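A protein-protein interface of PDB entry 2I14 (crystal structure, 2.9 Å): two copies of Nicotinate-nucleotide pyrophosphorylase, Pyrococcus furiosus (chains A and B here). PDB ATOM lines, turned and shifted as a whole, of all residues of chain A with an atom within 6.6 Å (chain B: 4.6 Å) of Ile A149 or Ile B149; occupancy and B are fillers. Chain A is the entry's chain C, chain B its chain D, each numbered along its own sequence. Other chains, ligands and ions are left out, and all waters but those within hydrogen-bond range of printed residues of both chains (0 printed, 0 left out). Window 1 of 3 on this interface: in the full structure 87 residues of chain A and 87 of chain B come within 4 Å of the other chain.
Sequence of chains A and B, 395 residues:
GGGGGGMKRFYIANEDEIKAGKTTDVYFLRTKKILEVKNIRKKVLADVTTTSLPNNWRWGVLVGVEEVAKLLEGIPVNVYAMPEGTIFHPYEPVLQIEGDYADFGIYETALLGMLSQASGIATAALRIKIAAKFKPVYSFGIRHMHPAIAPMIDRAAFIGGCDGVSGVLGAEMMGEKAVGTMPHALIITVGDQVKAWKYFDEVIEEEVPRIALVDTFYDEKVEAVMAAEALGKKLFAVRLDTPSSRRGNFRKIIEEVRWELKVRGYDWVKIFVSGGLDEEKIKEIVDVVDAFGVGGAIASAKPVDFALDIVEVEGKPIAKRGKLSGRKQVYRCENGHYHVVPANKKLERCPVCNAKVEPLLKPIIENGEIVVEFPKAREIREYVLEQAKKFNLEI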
ATOM      1  N   TYR A  11       5.313  26.092 -13.695  1.00  0.00           N
ATOM      2  CA  TYR A  11       5.977  27.278 -13.174  1.00  0.00           C
ATOM      3  C   TYR A  11       7.088  26.958 -12.200  1.00  0.00           C
ATOM      4  O   TYR A  11       7.033  27.364 -11.044  1.00  0.00           O
ATOM      5  CB  TYR A  11       4.981  28.195 -12.482  1.00  0.00           C
ATOM      6  CG  TYR A  11       3.985  28.843 -13.397  1.00  0.00           C
ATOM      7  CD1 TYR A  11       2.857  28.152 -13.840  1.00  0.00           C
ATOM      8  CD2 TYR A  11       4.148  30.168 -13.792  1.00  0.00           C
ATOM      9  CE1 TYR A  11       1.905  28.772 -14.652  1.00  0.00           C
ATOM     10  CE2 TYR A  11       3.207  30.802 -14.606  1.00  0.00           C
ATOM     11  CZ  TYR A  11       2.083  30.104 -15.030  1.00  0.00           C
ATOM     12  OH  TYR A  11       1.136  30.745 -15.807  1.00  0.00           O
ATOM     13  N   ILE A  12       8.097  26.234 -12.666  1.00  0.00           N
ATOM     14  CA  ILE A  12       9.231  25.878 -11.826  1.00  0.00           C
ATOM     15  C   ILE A  12      10.467  26.487 -12.443  1.00  0.00           C
ATOM     16  O   ILE A  12      10.390  27.090 -13.507  1.00  0.00           O
ATOM     17  CB  ILE A  12       9.415  24.350 -11.727  1.00  0.00           C
ATOM     18  CG1 ILE A  12       9.023  23.687 -13.049  1.00  0.00           C
ATOM     19  CG2 ILE A  12       8.562  23.794 -10.609  1.00  0.00           C
ATOM     20  CD1 ILE A  12       9.792  24.182 -14.282  1.00  0.00           C
ATOM     21  N   ALA A  13      11.604  26.342 -11.777  1.00  0.00           N
ATOM     22  CA  ALA A  13      12.846  26.883 -12.295  1.00  0.00           C
ATOM     23  C   ALA A  13      13.708  25.713 -12.694  1.00  0.00           C
ATOM     24  O   ALA A  13      13.755  24.721 -11.981  1.00  0.00           O
ATOM     25  CB  ALA A  13      13.552  27.705 -11.228  1.00  0.00           C
ATOM     26  N   ILE A  18      18.481  28.443 -11.983  1.00  0.00           N
ATOM     27  CA  ILE A  18      18.805  28.595 -10.576  1.00  0.00           C
ATOM     28  C   ILE A  18      20.299  28.817 -10.430  1.00  0.00           C
ATOM     29  O   ILE A  18      20.729  29.752  -9.757  1.00  0.00           O
ATOM     30  CB  ILE A  18      18.393  27.345  -9.766  1.00  0.00           C
ATOM     31  CG1 ILE A  18      16.872  27.182  -9.802  1.00  0.00           C
ATOM     32  CG2 ILE A  18      18.869  27.477  -8.330  1.00  0.00           C
ATOM     33  CD1 ILE A  18      16.371  25.968  -9.070  1.00  0.00           C
ATOM     34  N   GLN A 117      14.124  25.848   3.956  1.00  0.00           N
ATOM     35  CA  GLN A 117      13.039  24.879   3.948  1.00  0.00           C
ATOM     36  C   GLN A 117      13.489  23.464   4.323  1.00  0.00           C
ATOM     37  O   GLN A 117      12.770  22.731   5.010  1.00  0.00           O
ATOM     38  CB  GLN A 117      12.355  24.903   2.580  1.00  0.00           C
ATOM     39  CG  GLN A 117      10.976  24.266   2.554  1.00  0.00           C
ATOM     40  CD  GLN A 117      10.313  24.329   1.168  1.00  0.00           C
ATOM     41  OE1 GLN A 117       9.193  23.843   0.982  1.00  0.00           O
ATOM     42  NE2 GLN A 117      11.002  24.937   0.197  1.00  0.00           N
ATOM     43  N   ILE A 121      12.110  21.296   7.397  1.00  0.00           N
ATOM     44  CA  ILE A 121      11.555  19.956   7.372  1.00  0.00           C
ATOM     45  C   ILE A 121      12.335  18.987   8.255  1.00  0.00           C
ATOM     46  O   ILE A 121      11.749  18.167   8.977  1.00  0.00           O
ATOM     47  CB  ILE A 121      11.523  19.421   5.946  1.00  0.00           C
ATOM     48  CG1 ILE A 121      10.634  20.325   5.090  1.00  0.00           C
ATOM     49  CG2 ILE A 121      11.003  17.998   5.936  1.00  0.00           C
ATOM     50  CD1 ILE A 121      10.509  19.905   3.627  1.00  0.00           C
ATOM     51  N   ILE A 142       4.797  14.557   0.840  1.00  0.00           N
ATOM     52  CA  ILE A 142       4.983  15.256  -0.421  1.00  0.00           C
ATOM     53  C   ILE A 142       3.718  15.556  -1.224  1.00  0.00           C
ATOM     54  O   ILE A 142       3.755  16.335  -2.167  1.00  0.00           O
ATOM     55  CB  ILE A 142       6.005  14.544  -1.311  1.00  0.00           C
ATOM     56  CG1 ILE A 142       5.453  13.223  -1.823  1.00  0.00           C
ATOM     57  CG2 ILE A 142       7.274  14.310  -0.530  1.00  0.00           C
ATOM     58  CD1 ILE A 142       6.316  12.589  -2.894  1.00  0.00           C
ATOM     59  N   MET A 145       2.773  19.367  -1.129  1.00  0.00           N
ATOM     60  CA  MET A 145       3.634  20.404  -1.674  1.00  0.00           C
ATOM     61  C   MET A 145       3.870  20.159  -3.152  1.00  0.00           C
ATOM     62  O   MET A 145       3.491  19.121  -3.673  1.00  0.00           O
ATOM     63  CB  MET A 145       4.968  20.446  -0.929  1.00  0.00           C
ATOM     64  CG  MET A 145       4.859  20.619   0.583  1.00  0.00           C
ATOM     65  SD  MET A 145       4.360  22.232   1.144  1.00  0.00           S
ATOM     66  CE  MET A 145       5.961  23.072   1.168  1.00  0.00           C
ATOM     67  N   HIS A 146       4.494  21.123  -3.824  1.00  0.00           N
ATOM     68  CA  HIS A 146       4.781  21.015  -5.255  1.00  0.00           C
ATOM     69  C   HIS A 146       5.753  19.870  -5.550  1.00  0.00           C
ATOM     70  O   HIS A 146       6.809  19.756  -4.918  1.00  0.00           O
ATOM     71  CB  HIS A 146       5.384  22.328  -5.772  1.00  0.00           C
ATOM     72  CG  HIS A 146       5.339  22.473  -7.264  1.00  0.00           C
ATOM     73  ND1 HIS A 146       4.208  22.878  -7.940  1.00  0.00           N
ATOM     74  CD2 HIS A 146       6.277  22.231  -8.211  1.00  0.00           C
ATOM     75  CE1 HIS A 146       4.449  22.877  -9.238  1.00  0.00           C
ATOM     76  NE2 HIS A 146       5.698  22.488  -9.429  1.00  0.00           N
ATOM     77  N   PRO A 147       5.410  19.021  -6.536  1.00  0.00           N
ATOM     78  CA  PRO A 147       6.228  17.872  -6.946  1.00  0.00           C
ATOM     79  C   PRO A 147       7.655  18.238  -7.290  1.00  0.00           C
ATOM     80  O   PRO A 147       8.572  17.466  -7.052  1.00  0.00           O
ATOM     81  CB  PRO A 147       5.475  17.312  -8.145  1.00  0.00           C
ATOM     82  CG  PRO A 147       4.769  18.501  -8.695  1.00  0.00           C
ATOM     83  CD  PRO A 147       4.260  19.185  -7.440  1.00  0.00           C
ATOM     84  N   ALA A 148       7.851  19.423  -7.845  1.00  0.00           N
ATOM     85  CA  ALA A 148       9.195  19.838  -8.195  1.00  0.00           C
ATOM     86  C   ALA A 148      10.161  19.628  -7.018  1.00  0.00           C
ATOM     87  O   ALA A 148      11.331  19.278  -7.223  1.00  0.00           O
ATOM     88  CB  ALA A 148       9.193  21.288  -8.614  1.00  0.00           C
ATOM     89  N   ILE A 149       9.680  19.835  -5.788  1.00  0.00           N
ATOM     90  CA  ILE A 149      10.548  19.679  -4.626  1.00  0.00           C
ATOM     91  C   ILE A 149      10.355  18.350  -3.873  1.00  0.00           C
ATOM     92  O   ILE A 149      10.982  18.122  -2.821  1.00  0.00           O
ATOM     93  CB  ILE A 149      10.392  20.890  -3.652  1.00  0.00           C
ATOM     94  CG1 ILE A 149       8.922  21.061  -3.241  1.00  0.00           C
ATOM     95  CG2 ILE A 149      10.930  22.148  -4.319  1.00  0.00           C
ATOM     96  CD1 ILE A 149       8.692  22.047  -2.115  1.00  0.00           C
ATOM     97  N   ALA A 150       9.523  17.473  -4.437  1.00  0.00           N
ATOM     98  CA  ALA A 150       9.224  16.179  -3.834  1.00  0.00           C
ATOM     99  C   ALA A 150      10.458  15.508  -3.240  1.00  0.00           C
ATOM    100  O   ALA A 150      10.413  14.961  -2.128  1.00  0.00           O
ATOM    101  CB  ALA A 150       8.576  15.261  -4.867  1.00  0.00           C
ATOM    102  N   PRO A 151      11.574  15.517  -3.985  1.00  0.00           N
ATOM    103  CA  PRO A 151      12.784  14.896  -3.466  1.00  0.00           C
ATOM    104  C   PRO A 151      13.448  15.683  -2.333  1.00  0.00           C
ATOM    105  O   PRO A 151      13.694  15.118  -1.265  1.00  0.00           O
ATOM    106  CB  PRO A 151      13.669  14.757  -4.711  1.00  0.00           C
ATOM    107  CG  PRO A 151      13.244  15.854  -5.551  1.00  0.00           C
ATOM    108  CD  PRO A 151      11.741  15.830  -5.409  1.00  0.00           C
ATOM    109  N   MET A 152      13.726  16.968  -2.528  1.00  0.00           N
ATOM    110  CA  MET A 152      14.384  17.715  -1.457  1.00  0.00           C
ATOM    111  C   MET A 152      13.673  17.411  -0.146  1.00  0.00           C
ATOM    112  O   MET A 152      14.309  17.210   0.885  1.00  0.00           O
ATOM    113  CB  MET A 152      14.362  19.233  -1.712  1.00  0.00           C
ATOM    114  CG  MET A 152      13.227  19.974  -1.001  1.00  0.00           C
ATOM    115  SD  MET A 152      13.745  21.031   0.372  1.00  0.00           S
ATOM    116  CE  MET A 152      13.856  19.846   1.732  1.00  0.00           C
ATOM    117  N   ILE A 153      12.349  17.363  -0.198  1.00  0.00           N
ATOM    118  CA  ILE A 153      11.576  17.089   0.993  1.00  0.00           C
ATOM    119  C   ILE A 153      11.854  15.705   1.582  1.00  0.00           C
ATOM    120  O   ILE A 153      12.322  15.593   2.716  1.00  0.00           O
ATOM    121  CB  ILE A 153      10.072  17.232   0.726  1.00  0.00           C
ATOM    122  CG1 ILE A 153       9.767  18.668   0.325  1.00  0.00           C
ATOM    123  CG2 ILE A 153       9.273  16.838   1.975  1.00  0.00           C
ATOM    124  CD1 ILE A 153       8.307  18.929   0.113  1.00  0.00           C
ATOM    125  N   ASP A 154      11.564  14.651   0.830  1.00  0.00           N
ATOM    126  CA  ASP A 154      11.804  13.308   1.342  1.00  0.00           C
ATOM    127  C   ASP A 154      13.258  13.127   1.819  1.00  0.00           C
ATOM    128  O   ASP A 154      13.527  12.387   2.774  1.00  0.00           O
ATOM    129  CB  ASP A 154      11.456  12.254   0.285  1.00  0.00           C
ATOM    130  CG  ASP A 154       9.943  11.948   0.212  1.00  0.00           C
ATOM    131  OD1 ASP A 154       9.272  11.915   1.272  1.00  0.00           O
ATOM    132  OD2 ASP A 154       9.425  11.714  -0.910  1.00  0.00           O
ATOM    133  N   ALA A 299       6.550  17.651   5.870  1.00  0.00           N
ATOM    134  CA  ALA A 299       6.718  18.226   4.535  1.00  0.00           C
ATOM    135  C   ALA A 299       6.356  19.708   4.479  1.00  0.00           C
ATOM    136  O   ALA A 299       7.054  20.521   3.854  1.00  0.00           O
ATOM    137  CB  ALA A 299       5.883  17.471   3.546  1.00  0.00           C
ATOM    138  N   GLN B 117      -0.315  23.651  -2.297  1.00  0.00           N
ATOM    139  CA  GLN B 117       0.558  24.716  -1.852  1.00  0.00           C
ATOM    140  C   GLN B 117       0.232  26.064  -2.496  1.00  0.00           C
ATOM    141  O   GLN B 117       0.372  27.133  -1.863  1.00  0.00           O
ATOM    142  CB  GLN B 117       2.024  24.327  -2.105  1.00  0.00           C
ATOM    143  CG  GLN B 117       3.025  25.136  -1.335  1.00  0.00           C
ATOM    144  CD  GLN B 117       4.438  24.725  -1.619  1.00  0.00           C
ATOM    145  OE1 GLN B 117       5.376  25.296  -1.049  1.00  0.00           O
ATOM    146  NE2 GLN B 117       4.619  23.733  -2.503  1.00  0.00           N
ATOM    147  N   MET B 145      11.981  29.679   0.755  1.00  0.00           N
ATOM    148  CA  MET B 145      11.645  28.381   0.191  1.00  0.00           C
ATOM    149  C   MET B 145      12.629  27.997  -0.914  1.00  0.00           C
ATOM    150  O   MET B 145      13.480  28.798  -1.317  1.00  0.00           O
ATOM    151  CB  MET B 145      10.218  28.401  -0.353  1.00  0.00           C
ATOM    152  CG  MET B 145       9.153  28.831   0.666  1.00  0.00           C
ATOM    153  SD  MET B 145       8.738  27.599   1.946  1.00  0.00           S
ATOM    154  CE  MET B 145       7.544  26.529   1.054  1.00  0.00           C
ATOM    155  N   HIS B 146      12.511  26.767  -1.402  1.00  0.00           N
ATOM    156  CA  HIS B 146      13.394  26.283  -2.468  1.00  0.00           C
ATOM    157  C   HIS B 146      13.176  27.059  -3.774  1.00  0.00           C
ATOM    158  O   HIS B 146      12.036  27.227  -4.236  1.00  0.00           O
ATOM    159  CB  HIS B 146      13.157  24.789  -2.730  1.00  0.00           C
ATOM    160  CG  HIS B 146      14.268  24.129  -3.488  1.00  0.00           C
ATOM    161  ND1 HIS B 146      15.435  23.700  -2.887  1.00  0.00           N
ATOM    162  CD2 HIS B 146      14.401  23.844  -4.804  1.00  0.00           C
ATOM    163  CE1 HIS B 146      16.235  23.176  -3.798  1.00  0.00           C
ATOM    164  NE2 HIS B 146      15.632  23.251  -4.970  1.00  0.00           N
ATOM    165  N   PRO B 147      14.272  27.535  -4.388  1.00  0.00           N
ATOM    166  CA  PRO B 147      14.230  28.298  -5.643  1.00  0.00           C
ATOM    167  C   PRO B 147      13.484  27.588  -6.767  1.00  0.00           C
ATOM    168  O   PRO B 147      12.886  28.233  -7.643  1.00  0.00           O
ATOM    169  CB  PRO B 147      15.704  28.508  -5.968  1.00  0.00           C
ATOM    170  CG  PRO B 147      16.369  27.315  -5.328  1.00  0.00           C
ATOM    171  CD  PRO B 147      15.664  27.247  -4.002  1.00  0.00           C
ATOM    172  N   ALA B 148      13.510  26.259  -6.742  1.00  0.00           N
ATOM    173  CA  ALA B 148      12.824  25.505  -7.774  1.00  0.00           C
ATOM    174  C   ALA B 148      11.385  25.973  -7.901  1.00  0.00           C
ATOM    175  O   ALA B 148      10.849  26.058  -8.996  1.00  0.00           O
ATOM    176  CB  ALA B 148      12.859  24.031  -7.461  1.00  0.00           C
ATOM    177  N   ILE B 149      10.761  26.295  -6.777  1.00  0.00           N
ATOM    178  CA  ILE B 149       9.376  26.736  -6.814  1.00  0.00           C
ATOM    179  C   ILE B 149       9.180  28.250  -6.721  1.00  0.00           C
ATOM    180  O   ILE B 149       8.052  28.734  -6.644  1.00  0.00           O
ATOM    181  CB  ILE B 149       8.550  26.031  -5.719  1.00  0.00           C
ATOM    182  CG1 ILE B 149       9.172  26.279  -4.342  1.00  0.00           C
ATOM    183  CG2 ILE B 149       8.484  24.541  -6.016  1.00  0.00           C
ATOM    184  CD1 ILE B 149       8.301  25.794  -3.179  1.00  0.00           C
ATOM    185  N   ALA B 150      10.287  28.991  -6.769  1.00  0.00           N
ATOM    186  CA  ALA B 150      10.269  30.459  -6.703  1.00  0.00           C
ATOM    187  C   ALA B 150       9.124  31.073  -7.519  1.00  0.00           C
ATOM    188  O   ALA B 150       8.400  31.962  -7.049  1.00  0.00           O
ATOM    189  CB  ALA B 150      11.618  31.025  -7.189  1.00  0.00           C
ATOM    190  N   PRO B 151       8.954  30.613  -8.766  1.00  0.00           N
ATOM    191  CA  PRO B 151       7.883  31.157  -9.580  1.00  0.00           C
ATOM    192  C   PRO B 151       6.499  30.739  -9.141  1.00  0.00           C
ATOM    193  O   PRO B 151       5.650  31.600  -8.963  1.00  0.00           O
ATOM    194  CB  PRO B 151       8.231  30.666 -10.974  1.00  0.00           C
ATOM    195  CG  PRO B 151       8.933  29.393 -10.713  1.00  0.00           C
ATOM    196  CD  PRO B 151       9.833  29.750  -9.577  1.00  0.00           C
ATOM    197  N   MET B 152       6.248  29.449  -8.947  1.00  0.00           N
ATOM    198  CA  MET B 152       4.886  29.046  -8.562  1.00  0.00           C
ATOM    199  C   MET B 152       4.413  29.930  -7.425  1.00  0.00           C
ATOM    200  O   MET B 152       3.263  30.389  -7.396  1.00  0.00           O
ATOM    201  CB  MET B 152       4.816  27.578  -8.115  1.00  0.00           C
ATOM    202  CG  MET B 152       4.916  27.371  -6.591  1.00  0.00           C
ATOM    203  SD  MET B 152       3.387  26.848  -5.769  1.00  0.00           S
ATOM    204  CE  MET B 152       2.485  28.340  -5.581  1.00  0.00           C
ATOM    205  N   ILE B 153       5.324  30.182  -6.497  1.00  0.00           N
ATOM    206  CA  ILE B 153       5.011  31.002  -5.345  1.00  0.00           C
ATOM    207  C   ILE B 153       4.639  32.414  -5.731  1.00  0.00           C
ATOM    208  O   ILE B 153       3.508  32.825  -5.494  1.00  0.00           O
ATOM    209  CB  ILE B 153       6.182  31.041  -4.337  1.00  0.00           C
ATOM    210  CG1 ILE B 153       6.443  29.631  -3.795  1.00  0.00           C
ATOM    211  CG2 ILE B 153       5.842  31.995  -3.176  1.00  0.00           C
ATOM    212  CD1 ILE B 153       7.539  29.578  -2.760  1.00  0.00           C
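NE2 of Gln B117 sits close to N of His A146. The backbone NH (N) of Ala A13 sits at hydrogen-bond distance from the backbone carbonyl oxygen (O) of Ala B148, at 2.9 Å. The side-chain amide nitrogen (NE2) of Gln A117 sits close to the backbone NH (N) of His B146, at 2.9 Å. O of Tyr A11 sits at hydrogen-bond distance from N of Met B152, 3.1 Å away.
Tyr A11 touches Pro B151 (O to CG, 2.8 Å). O of Ala B148 touches CA of Ile A12 (3.3 Å). Pro B151 touches Ile A12 (CG to CA, 3.7 Å). Ala A13 touches Pro B147 (CB to O, 3.7 Å). Ala B148 touches Ile A18 (N to CD1, 3.7 Å). Met B145 touches Gln A117 (CE to OE1, 3.2 Å). Met B145 touches Met A145. Ile B149 touches His A146 (CG2 to CB, 3.8 Å). Ile A149 touches His B146. Ile A149 touches Ile B149.
Of chain B, only His B146 and Ile B149 come within 4 Å of Ile A149. Of chain A, only His A146 (3.8 Å) and Ile A149 (3.8 Å) come within 4 Å of Ile B149. Of the printed residues of chain B, Ile A18 touches Pro B147 (3.9 Å) and Ala B148 (3.7 Å). Printed residues of chain A within 4 Å of Met B145: Gln A117 and Met A145. Of the printed residues of chain A, Gln B117 touches Met A145 and His A146. Pro A147 touches none of the printed residues of chain B. Ile A142 touches none of the printed residues of chain B. The nearest residue of chain B that does not touch Ile A149 is Ala B148 (4.1 Å).
Of the 10 printed residues of chain B, 8 touch a printed residue of chain A. Printed residues of chain B that touch a printed residue of chain A: Gln B117, Met B145, His B146, Pro B147, Ala B148, Ile B149, Pro B151 and Met B152. Among the printed residues, no Asp or Glu carboxylate lies within 4 Å of a Lys or Arg side-chain nitrogen of the other chain.
Gln A117 touches Met B145, and with the chains exchanged Met A145 touches Gln B117. Gln A117 touches His B146, and with the chains exchanged His A146 touches Gln B117. Met A145 touches its own counterpart, Met B145. Ile A149 touches its own counterpart, Ile B149. 10 positions are printed for both chains. Of the 16 pairs that touch across the chains among the printed residues, 8 have their exchanged pair printed and touching as well.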
